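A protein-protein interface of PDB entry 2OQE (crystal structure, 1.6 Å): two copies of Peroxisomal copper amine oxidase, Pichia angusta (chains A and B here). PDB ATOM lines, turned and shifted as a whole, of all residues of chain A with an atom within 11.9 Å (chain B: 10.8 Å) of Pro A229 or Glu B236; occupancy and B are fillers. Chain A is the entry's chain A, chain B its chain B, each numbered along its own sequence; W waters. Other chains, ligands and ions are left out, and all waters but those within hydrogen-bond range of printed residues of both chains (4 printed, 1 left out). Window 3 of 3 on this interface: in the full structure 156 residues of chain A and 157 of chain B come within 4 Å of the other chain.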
ATOM      1  N   PRO A 225      14.863 -33.792  27.177  1.00  0.00           N
ATOM      2  CA  PRO A 225      14.509 -32.376  27.046  1.00  0.00           C
ATOM      3  C   PRO A 225      14.115 -32.050  25.609  1.00  0.00           C
ATOM      4  O   PRO A 225      14.570 -32.726  24.678  1.00  0.00           O
ATOM      5  CB  PRO A 225      15.819 -31.647  27.390  1.00  0.00           C
ATOM      6  CG  PRO A 225      16.614 -32.604  28.181  1.00  0.00           C
ATOM      7  CD  PRO A 225      16.229 -33.984  27.703  1.00  0.00           C
ATOM      8  N   GLU A 226      13.267 -31.043  25.427  1.00  0.00           N
ATOM      9  CA  GLU A 226      12.950 -30.543  24.096  1.00  0.00           C
ATOM     10  C   GLU A 226      14.261 -30.121  23.430  1.00  0.00           C
ATOM     11  O   GLU A 226      15.032 -29.348  23.999  1.00  0.00           O
ATOM     12  CB  GLU A 226      12.020 -29.336  24.197  1.00  0.00           C
ATOM     13  CG  GLU A 226      11.450 -28.838  22.869  1.00  0.00           C
ATOM     14  CD  GLU A 226      10.010 -29.265  22.667  1.00  0.00           C
ATOM     15  OE1 GLU A 226       9.157 -28.894  23.510  1.00  0.00           O
ATOM     16  OE2 GLU A 226       9.730 -29.973  21.670  1.00  0.00           O
ATOM     17  N   ALA A 227      14.516 -30.648  22.237  1.00  0.00           N
ATOM     18  CA  ALA A 227      15.677 -30.231  21.454  1.00  0.00           C
ATOM     19  C   ALA A 227      15.488 -28.795  20.992  1.00  0.00           C
ATOM     20  O   ALA A 227      14.351 -28.350  20.801  1.00  0.00           O
ATOM     21  CB  ALA A 227      15.888 -31.161  20.253  1.00  0.00           C
ATOM     22  N   PRO A 228      16.601 -28.051  20.832  1.00  0.00           N
ATOM     23  CA  PRO A 228      16.496 -26.724  20.230  1.00  0.00           C
ATOM     24  C   PRO A 228      15.896 -26.809  18.826  1.00  0.00           C
ATOM     25  O   PRO A 228      16.171 -27.770  18.096  1.00  0.00           O
ATOM     26  CB  PRO A 228      17.949 -26.236  20.178  1.00  0.00           C
ATOM     27  CG  PRO A 228      18.790 -27.434  20.374  1.00  0.00           C
ATOM     28  CD  PRO A 228      17.991 -28.384  21.199  1.00  0.00           C
ATOM     29  N   PRO A 229      15.063 -25.825  18.457  1.00  0.00           N
ATOM     30  CA  PRO A 229      14.314 -25.881  17.208  1.00  0.00           C
ATOM     31  C   PRO A 229      15.173 -25.738  15.951  1.00  0.00           C
ATOM     32  O   PRO A 229      16.206 -25.066  15.971  1.00  0.00           O
ATOM     33  CB  PRO A 229      13.360 -24.684  17.330  1.00  0.00           C
ATOM     34  CG  PRO A 229      14.077 -23.729  18.193  1.00  0.00           C
ATOM     35  CD  PRO A 229      14.768 -24.588  19.210  1.00  0.00           C
ATOM     36  N   ILE A 230      14.743 -26.401  14.882  1.00  0.00           N
ATOM     37  CA  ILE A 230      15.240 -26.141  13.541  1.00  0.00           C
ATOM     38  C   ILE A 230      14.077 -25.484  12.793  1.00  0.00           C
ATOM     39  O   ILE A 230      13.067 -26.127  12.528  1.00  0.00           O
ATOM     40  CB  ILE A 230      15.678 -27.440  12.811  1.00  0.00           C
ATOM     41  CG1 ILE A 230      16.712 -28.206  13.646  1.00  0.00           C
ATOM     42  CG2 ILE A 230      16.226 -27.113  11.412  1.00  0.00           C
ATOM     43  CD1 ILE A 230      16.946 -29.655  13.201  1.00  0.00           C
ATOM     44  N   ASN A 231      14.206 -24.196  12.483  1.00  0.00           N
ATOM     45  CA  ASN A 231      13.101 -23.455  11.879  1.00  0.00           C
ATOM     46  C   ASN A 231      13.245 -23.309  10.372  1.00  0.00           C
ATOM     47  O   ASN A 231      14.324 -22.994   9.880  1.00  0.00           O
ATOM     48  CB  ASN A 231      12.934 -22.083  12.552  1.00  0.00           C
ATOM     49  CG  ASN A 231      12.526 -22.195  14.015  1.00  0.00           C
ATOM     50  OD1 ASN A 231      11.750 -23.074  14.394  1.00  0.00           O
ATOM     51  ND2 ASN A 231      13.045 -21.297  14.839  1.00  0.00           N
ATOM     52  N   VAL A 232      12.154 -23.556   9.653  1.00  0.00           N
ATOM     53  CA  VAL A 232      12.134 -23.451   8.199  1.00  0.00           C
ATOM     54  C   VAL A 232      11.129 -22.379   7.799  1.00  0.00           C
ATOM     55  O   VAL A 232       9.941 -22.465   8.121  1.00  0.00           O
ATOM     56  CB  VAL A 232      11.781 -24.807   7.527  1.00  0.00           C
ATOM     57  CG1 VAL A 232      11.709 -24.654   6.014  1.00  0.00           C
ATOM     58  CG2 VAL A 232      12.812 -25.868   7.894  1.00  0.00           C
ATOM     59  N   THR A 233      11.617 -21.363   7.098  1.00  0.00           N
ATOM     60  CA  THR A 233      10.781 -20.243   6.700  1.00  0.00           C
ATOM     61  C   THR A 233      10.977 -19.939   5.224  1.00  0.00           C
ATOM     62  O   THR A 233      12.055 -20.166   4.674  1.00  0.00           O
ATOM     63  CB  THR A 233      11.132 -18.982   7.500  1.00  0.00           C
ATOM     64  OG1 THR A 233      12.547 -18.785   7.458  1.00  0.00           O
ATOM     65  CG2 THR A 233      10.686 -19.125   8.962  1.00  0.00           C
ATOM     66  N   GLY A 323       1.267 -27.600  12.372  1.00  0.00           N
ATOM     67  CA  GLY A 323       2.048 -27.986  11.204  1.00  0.00           C
ATOM     68  C   GLY A 323       3.091 -28.951  11.738  1.00  0.00           C
ATOM     69  O   GLY A 323       4.256 -28.582  11.919  1.00  0.00           O
ATOM     70  N   LYS A 327       6.253 -29.867   7.637  1.00  0.00           N
ATOM     71  CA  LYS A 327       6.974 -28.709   8.141  1.00  0.00           C
ATOM     72  C   LYS A 327       7.256 -27.690   7.037  1.00  0.00           C
ATOM     73  O   LYS A 327       7.666 -28.057   5.936  1.00  0.00           O
ATOM     74  CB  LYS A 327       8.282 -29.188   8.765  1.00  0.00           C
ATOM     75  CG  LYS A 327       9.006 -28.160   9.584  1.00  0.00           C
ATOM     76  CD  LYS A 327      10.141 -28.818  10.324  1.00  0.00           C
ATOM     77  CE  LYS A 327      10.891 -27.811  11.152  1.00  0.00           C
ATOM     78  NZ  LYS A 327      11.787 -28.517  12.107  1.00  0.00           N
ATOM     79  N   GLY A 328       7.042 -26.414   7.344  1.00  0.00           N
ATOM     80  CA  GLY A 328       7.289 -25.338   6.383  1.00  0.00           C
ATOM     81  C   GLY A 328       6.006 -24.701   5.887  1.00  0.00           C
ATOM     82  O   GLY A 328       4.960 -24.813   6.533  1.00  0.00           O
ATOM     83  N   ASN B 231      14.717 -20.585   4.101  1.00  0.00           N
ATOM     84  CA  ASN B 231      15.687 -20.286   5.155  1.00  0.00           C
ATOM     85  C   ASN B 231      15.661 -21.297   6.290  1.00  0.00           C
ATOM     86  O   ASN B 231      14.590 -21.660   6.771  1.00  0.00           O
ATOM     87  CB  ASN B 231      15.474 -18.864   5.696  1.00  0.00           C
ATOM     88  CG  ASN B 231      15.804 -17.791   4.667  1.00  0.00           C
ATOM     89  OD1 ASN B 231      16.733 -17.936   3.867  1.00  0.00           O
ATOM     90  ND2 ASN B 231      15.047 -16.702   4.694  1.00  0.00           N
ATOM     91  N   VAL B 232      16.843 -21.746   6.710  1.00  0.00           N
ATOM     92  CA  VAL B 232      16.967 -22.700   7.813  1.00  0.00           C
ATOM     93  C   VAL B 232      17.740 -22.068   8.964  1.00  0.00           C
ATOM     94  O   VAL B 232      18.901 -21.675   8.807  1.00  0.00           O
ATOM     95  CB  VAL B 232      17.643 -24.023   7.365  1.00  0.00           C
ATOM     96  CG1 VAL B 232      17.790 -24.974   8.539  1.00  0.00           C
ATOM     97  CG2 VAL B 232      16.826 -24.689   6.265  1.00  0.00           C
ATOM     98  N   THR B 233      17.091 -21.974  10.120  1.00  0.00           N
ATOM     99  CA  THR B 233      17.689 -21.334  11.284  1.00  0.00           C
ATOM    100  C   THR B 233      17.564 -22.215  12.518  1.00  0.00           C
ATOM    101  O   THR B 233      16.598 -22.966  12.665  1.00  0.00           O
ATOM    102  CB  THR B 233      16.999 -20.001  11.600  1.00  0.00           C
ATOM    103  OG1 THR B 233      15.584 -20.205  11.631  1.00  0.00           O
ATOM    104  CG2 THR B 233      17.324 -18.949  10.539  1.00  0.00           C
ATOM    105  N   GLN B 234      18.554 -22.105  13.399  1.00  0.00           N
ATOM    106  CA  GLN B 234      18.519 -22.748  14.701  1.00  0.00           C
ATOM    107  C   GLN B 234      18.816 -21.683  15.752  1.00  0.00           C
ATOM    108  O   GLN B 234      19.915 -21.640  16.292  1.00  0.00           O
ATOM    109  CB  GLN B 234      19.535 -23.893  14.772  1.00  0.00           C
ATOM    110  CG  GLN B 234      19.165 -25.099  13.898  1.00  0.00           C
ATOM    111  CD  GLN B 234      20.019 -26.320  14.200  1.00  0.00           C
ATOM    112  OE1 GLN B 234      20.944 -26.623  13.463  1.00  0.00           O
ATOM    113  NE2 GLN B 234      19.726 -27.008  15.308  1.00  0.00           N
ATOM    114  N   PRO B 235      17.816 -20.823  16.045  1.00  0.00           N
ATOM    115  CA  PRO B 235      18.015 -19.657  16.910  1.00  0.00           C
ATOM    116  C   PRO B 235      18.486 -19.960  18.337  1.00  0.00           C
ATOM    117  O   PRO B 235      19.048 -19.077  18.990  1.00  0.00           O
ATOM    118  CB  PRO B 235      16.628 -18.995  16.928  1.00  0.00           C
ATOM    119  CG  PRO B 235      15.677 -20.066  16.562  1.00  0.00           C
ATOM    120  CD  PRO B 235      16.422 -20.910  15.572  1.00  0.00           C
ATOM    121  N   GLU B 236      18.246 -21.179  18.814  1.00  0.00           N
ATOM    122  CA  GLU B 236      18.673 -21.593  20.152  1.00  0.00           C
ATOM    123  C   GLU B 236      19.878 -22.544  20.113  1.00  0.00           C
ATOM    124  O   GLU B 236      20.173 -23.229  21.096  1.00  0.00           O
ATOM    125  CB  GLU B 236      17.513 -22.249  20.911  1.00  0.00           C
ATOM    126  CG  GLU B 236      16.333 -21.315  21.180  1.00  0.00           C
ATOM    127  CD  GLU B 236      15.194 -22.001  21.927  1.00  0.00           C
ATOM    128  OE1 GLU B 236      15.456 -22.665  22.961  1.00  0.00           O
ATOM    129  OE2 GLU B 236      14.030 -21.868  21.483  1.00  0.00           O
ATOM    130  N   GLY B 237      20.561 -22.578  18.972  1.00  0.00           N
ATOM    131  CA  GLY B 237      21.716 -23.453  18.788  1.00  0.00           C
ATOM    132  C   GLY B 237      21.370 -24.886  18.418  1.00  0.00           C
ATOM    133  O   GLY B 237      20.232 -25.202  18.066  1.00  0.00           O
ATOM    134  N   VAL B 238      22.378 -25.752  18.495  1.00  0.00           N
ATOM    135  CA  VAL B 238      22.259 -27.142  18.062  1.00  0.00           C
ATOM    136  C   VAL B 238      22.177 -28.081  19.250  1.00  0.00           C
ATOM    137  O   VAL B 238      22.543 -27.706  20.366  1.00  0.00           O
ATOM    138  CB  VAL B 238      23.450 -27.551  17.171  1.00  0.00           C
ATOM    139  CG1 VAL B 238      23.543 -26.621  15.985  1.00  0.00           C
ATOM    140  CG2 VAL B 238      24.770 -27.570  17.965  1.00  0.00           C
ATOM    141  N   SER B 239      21.711 -29.305  19.006  1.00  0.00           N
ATOM    142  CA  SER B 239      21.574 -30.291  20.066  1.00  0.00           C
ATOM    143  C   SER B 239      22.830 -31.144  20.237  1.00  0.00           C
ATOM    144  O   SER B 239      22.961 -31.860  21.232  1.00  0.00           O
ATOM    145  CB  SER B 239      20.365 -31.198  19.812  1.00  0.00           C
ATOM    146  OG  SER B 239      20.682 -32.192  18.844  1.00  0.00           O
ATOM    147  N   PHE B 240      23.740 -31.099  19.267  1.00  0.00           N
ATOM    148  CA  PHE B 240      24.962 -31.887  19.408  1.00  0.00           C
ATOM    149  C   PHE B 240      26.043 -31.132  20.170  1.00  0.00           C
ATOM    150  O   PHE B 240      26.018 -29.898  20.260  1.00  0.00           O
ATOM    151  CB  PHE B 240      25.478 -32.421  18.070  1.00  0.00           C
ATOM    152  CG  PHE B 240      25.888 -31.363  17.086  1.00  0.00           C
ATOM    153  CD1 PHE B 240      25.005 -30.927  16.114  1.00  0.00           C
ATOM    154  CD2 PHE B 240      27.192 -30.838  17.096  1.00  0.00           C
ATOM    155  CE1 PHE B 240      25.398 -29.965  15.167  1.00  0.00           C
ATOM    156  CE2 PHE B 240      27.588 -29.894  16.172  1.00  0.00           C
ATOM    157  CZ  PHE B 240      26.693 -29.446  15.208  1.00  0.00           C
ATOM    158  N   GLY B 328      22.620 -24.213   6.782  1.00  0.00           N
ATOM    159  CA  GLY B 328      22.238 -24.246   8.191  1.00  0.00           C
ATOM    160  C   GLY B 328      23.380 -23.870   9.110  1.00  0.00           C
ATOM    161  O   GLY B 328      24.343 -23.218   8.689  1.00  0.00           O
ATOM    162  N   VAL B 329      23.259 -24.273  10.371  1.00  0.00           N
ATOM    163  CA  VAL B 329      24.275 -24.008  11.381  1.00  0.00           C
ATOM    164  C   VAL B 329      25.303 -25.140  11.342  1.00  0.00           C
ATOM    165  O   VAL B 329      24.990 -26.291  11.641  1.00  0.00           O
ATOM    166  CB  VAL B 329      23.655 -23.860  12.793  1.00  0.00           C
ATOM    167  CG1 VAL B 329      24.743 -23.710  13.848  1.00  0.00           C
ATOM    168  CG2 VAL B 329      22.719 -22.647  12.823  1.00  0.00           C
ATOM    169  N   GLU B 355      23.094 -30.800  12.012  1.00  0.00           N
ATOM    170  CA  GLU B 355      21.869 -31.575  12.164  1.00  0.00           C
ATOM    171  C   GLU B 355      20.773 -30.995  11.272  1.00  0.00           C
ATOM    172  O   GLU B 355      20.726 -29.792  11.034  1.00  0.00           O
ATOM    173  CB  GLU B 355      21.445 -31.701  13.638  1.00  0.00           C
ATOM    174  CG  GLU B 355      21.025 -30.397  14.322  1.00  0.00           C
ATOM    175  CD  GLU B 355      20.842 -30.544  15.829  1.00  0.00           C
ATOM    176  OE1 GLU B 355      20.955 -31.677  16.358  1.00  0.00           O
ATOM    177  OE2 GLU B 355      20.579 -29.516  16.487  1.00  0.00           O
ATOM    178  N   GLU B 356      19.919 -31.866  10.749  1.00  0.00           N
ATOM    179  CA  GLU B 356      18.868 -31.465   9.822  1.00  0.00           C
ATOM    180  C   GLU B 356      17.572 -32.175  10.178  1.00  0.00           C
ATOM    181  O   GLU B 356      17.593 -33.274  10.731  1.00  0.00           O
ATOM    182  CB  GLU B 356      19.207 -31.884   8.396  1.00  0.00           C
ATOM    183  CG  GLU B 356      20.550 -31.439   7.854  1.00  0.00           C
ATOM    184  CD  GLU B 356      20.744 -31.915   6.428  1.00  0.00           C
ATOM    185  OE1 GLU B 356      19.738 -32.002   5.694  1.00  0.00           O
ATOM    186  OE2 GLU B 356      21.892 -32.220   6.044  1.00  0.00           O
ATOM    187  N   ASP B 357      16.446 -31.554   9.837  1.00  0.00           N
ATOM    188  CA  ASP B 357      15.164 -32.236   9.937  1.00  0.00           C
ATOM    189  C   ASP B 357      15.172 -33.408   8.957  1.00  0.00           C
ATOM    190  O   ASP B 357      15.728 -33.327   7.859  1.00  0.00           O
ATOM    191  CB  ASP B 357      13.996 -31.285   9.653  1.00  0.00           C
ATOM    192  CG  ASP B 357      12.630 -31.963   9.839  1.00  0.00           C
ATOM    193  OD1 ASP B 357      12.214 -32.233  10.997  1.00  0.00           O
ATOM    194  OD2 ASP B 357      11.975 -32.246   8.817  1.00  0.00           O
ATOM    195  N   ARG B 378       8.752 -36.052  15.058  1.00  0.00           N
ATOM    196  CA  ARG B 378       9.595 -35.714  13.915  1.00  0.00           C
ATOM    197  C   ARG B 378      11.030 -36.161  14.173  1.00  0.00           C
ATOM    198  O   ARG B 378      11.484 -36.198  15.325  1.00  0.00           O
ATOM    199  CB  ARG B 378       9.529 -34.219  13.612  1.00  0.00           C
ATOM    200  CG  ARG B 378       8.138 -33.762  13.131  1.00  0.00           C
ATOM    201  CD  ARG B 378       8.193 -32.392  12.447  1.00  0.00           C
ATOM    202  NE  ARG B 378       8.949 -32.435  11.194  1.00  0.00           N
ATOM    203  CZ  ARG B 378       8.435 -32.744  10.007  1.00  0.00           C
ATOM    204  NH1 ARG B 378       7.145 -33.044   9.884  1.00  0.00           N
ATOM    205  NH2 ARG B 378       9.212 -32.758   8.934  1.00  0.00           N
ATOM    206  N   ALA B 379      11.714 -36.507  13.080  1.00  0.00           N
ATOM    207  CA  ALA B 379      13.082 -37.015  13.113  1.00  0.00           C
ATOM    208  C   ALA B 379      14.090 -35.906  12.885  1.00  0.00           C
ATOM    209  O   ALA B 379      13.877 -35.007  12.074  1.00  0.00           O
ATOM    210  CB  ALA B 379      13.273 -38.073  12.037  1.00  0.00           C
ATOM    211  N   THR B 380      15.214 -36.012  13.573  1.00  0.00           N
ATOM    212  CA  THR B 380      16.369 -35.193  13.265  1.00  0.00           C
ATOM    213  C   THR B 380      17.509 -36.139  12.877  1.00  0.00           C
ATOM    214  O   THR B 380      17.642 -37.236  13.438  1.00  0.00           O
ATOM    215  CB  THR B 380      16.756 -34.314  14.476  1.00  0.00           C
ATOM    216  OG1 THR B 380      15.611 -33.530  14.865  1.00  0.00           O
ATOM    217  CG2 THR B 380      17.914 -33.373  14.134  1.00  0.00           C
ATOM    218  N   SER B 648       5.962 -34.220  18.386  1.00  0.00           N
ATOM    219  CA  SER B 648       5.544 -32.940  17.830  1.00  0.00           C
ATOM    220  C   SER B 648       4.064 -32.709  18.120  1.00  0.00           C
ATOM    221  O   SER B 648       3.599 -31.565  18.203  1.00  0.00           O
ATOM    222  CB  SER B 648       5.794 -32.905  16.322  1.00  0.00           C
ATOM    223  OG  SER B 648       7.184 -32.992  16.064  1.00  0.00           O
HETATM  224  O   HOH W   1      14.102 -19.852   9.399  1.00  0.00           O
HETATM  225  O   HOH W   2      13.101 -16.117   7.125  1.00  0.00           O
HETATM  226  O   HOH W   3      17.801 -29.995  17.437  1.00  0.00           O
HETATM  227  O   HOH W   4       7.753 -32.212   6.389  1.00  0.00           O
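O of Thr A233 sits at hydrogen-bond distance from N of Asn B231 (2.8 Å).
The backbone carbonyl oxygen (O) of Asn B231 lies close to the backbone carbonyl oxygen (O) of Asn A231.
The side-chain amino group of Lys A327 lies within salt-bridge range of the side-chain carboxylate of Asp B357 (3.9 Å).
The backbone carbonyl oxygen (O) of Thr B233 lies within hydrogen-bond range of the backbone NH (N) of Asn A231.
Asn B231 touches its own counterpart, Asn A231.
Asn A231 touches Val B232, and with the chains exchanged Val A232 touches Asn B231.
Asn A231 touches Thr B233, and with the chains exchanged Thr A233 touches Asn B231.
Of the 21 pairs that touch across the chains among the printed residues, 5 have their exchanged pair printed and touching as well.
Water W1 lies within hydrogen-bond range of OG1 of Thr B233 (2.7 Å), OG1 of Thr A233 (2.7 Å), O of Asn A231 (3.2 Å) and O of Asn B231 (3.2 Å).
Water W2 lies within hydrogen-bond range of the side-chain hydroxyl of Thr A233 (2.7 Å) and the side-chain amide nitrogen of Asn B231 (3.2 Å).
Water W3 lies within hydrogen-bond range of the backbone carbonyl oxygen (O) of Pro A228 and the side-chain carboxylate (OE2) of Glu B355.
Water W4 bridges NH2 of Arg B378 (3.0 Å) and N of Lys A327 (3.1 Å).
Among the printed residues, pairs that only touch across the chains: Pro A228 with Glu B236 (3.9 Å), Pro A228 with Gly B237 (3.3 Å), Pro A228 with Val B238 (3.6 Å), Pro A228 with Ser B239 (3.7 Å), Pro A229 with Thr B233 (3.9 Å), Pro A229 with Gln B234 (3.5 Å), Pro A229 with Glu B236 (3.6 Å), Ile A230 with Val B232 (3.9 Å), Ile A230 with Thr B233 (3.6 Å), Ile A230 with Gln B234 (3.6 Å), Ile A230 with Glu B356 (3.99 Å), Ile A230 with Asp B357 (3.9 Å), Ile A230 with Thr B380 (3.95 Å), Asn A231 with Val B232 (3.4 Å), Asn A231 with Pro B235 (3.4 Å), Val A232 with Asn B231 (3.4 Å) and Lys A327 with Arg B378 (3.7 Å).
Of the 12 printed residues of chain A, 7 touch a printed residue of chain B.
Hydrophobic or aromatic side chains of chain A that line the printed part of chain B: Pro A228, Pro A229 and Ile A230.
Along chain A the printed residues that touch a printed residue of chain B span positions 228 to 327.
Of the 19 printed residues of chain B, 13 touch a printed residue of chain A.
Hydrophobic or aromatic side chains of chain B that line the printed part of chain A: Val B232 and Pro B235.
Among the printed residues, Asp or Glu carboxylates within 4 Å of a Lys or Arg side-chain nitrogen of the other chain: Lys A327 with Asp B357.
OE1 of Glu B355 is in hydrogen-bond range of OG of Ser B239 (2.6 Å).
NE2 of Gln B234 is in hydrogen-bond range of OE2 of Glu B355, 2.9 Å away.
OD2 of Asp B357 lies within salt-bridge range of NH2 of Arg B378 (2.8 Å).
O of Gly B237 sits at hydrogen-bond distance from NE2 of Gln B234 (3.3 Å).
The backbone carbonyl oxygen (O) of Ile A230 sits at hydrogen-bond distance from the side-chain amino group (NZ) of Lys A327.
Pro A229 touches three residues of chain B.
Of chain A, only Pro A228 and Pro A229 come within 4 Å of Glu B236.
No residue of chain B comes within 4 Å of Ala A227.
Of chain B, only Glu B236, Gly B237, Val B238 and Ser B239 come within 4 Å of Pro A228.
Asn A231 touches just these residues of chain B: Asn B231, Val B232, Thr B233 and Pro B235.
Of chain A, only Pro A229 (3.5 Å) and Ile A230 (3.6 Å) come within 4 Å of Gln B234.
Gly B237 touches just one residue of chain A: Pro A228.
Of the printed residues of chain B, Ile A230 touches Val B232 (3.9 Å), Thr B233 (3.6 Å), Gln B234 (3.6 Å), Glu B356 (3.99 Å), Asp B357 (3.9 Å) and Thr B380 (3.95 Å).
Printed residues of chain A within 4 Å of Asp B357: Ile A230 (3.9 Å) and Lys A327 (3.9 Å).
Printed residues of chain B within 4 Å of Val A232: Asn B231 (3.4 Å).
Of the printed residues of chain B, Thr A233 touches Asn B231 (2.8 Å).
Of the printed residues of chain A, Asn B231 touches Asn A231 (3.4 Å), Val A232 (3.4 Å) and Thr A233 (2.8 Å).
Gly A323 touches none of the printed residues of chain B.
The nearest residue of chain B that does not touch Pro A229 is Pro B235 (4.2 Å).
The nearest residue of chain A that does not touch Glu B236 is Ala A227 (6.2 Å).
The nearest printed residue of chain A that does not touch Asn B231 is Ile A230 (7.2 Å).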
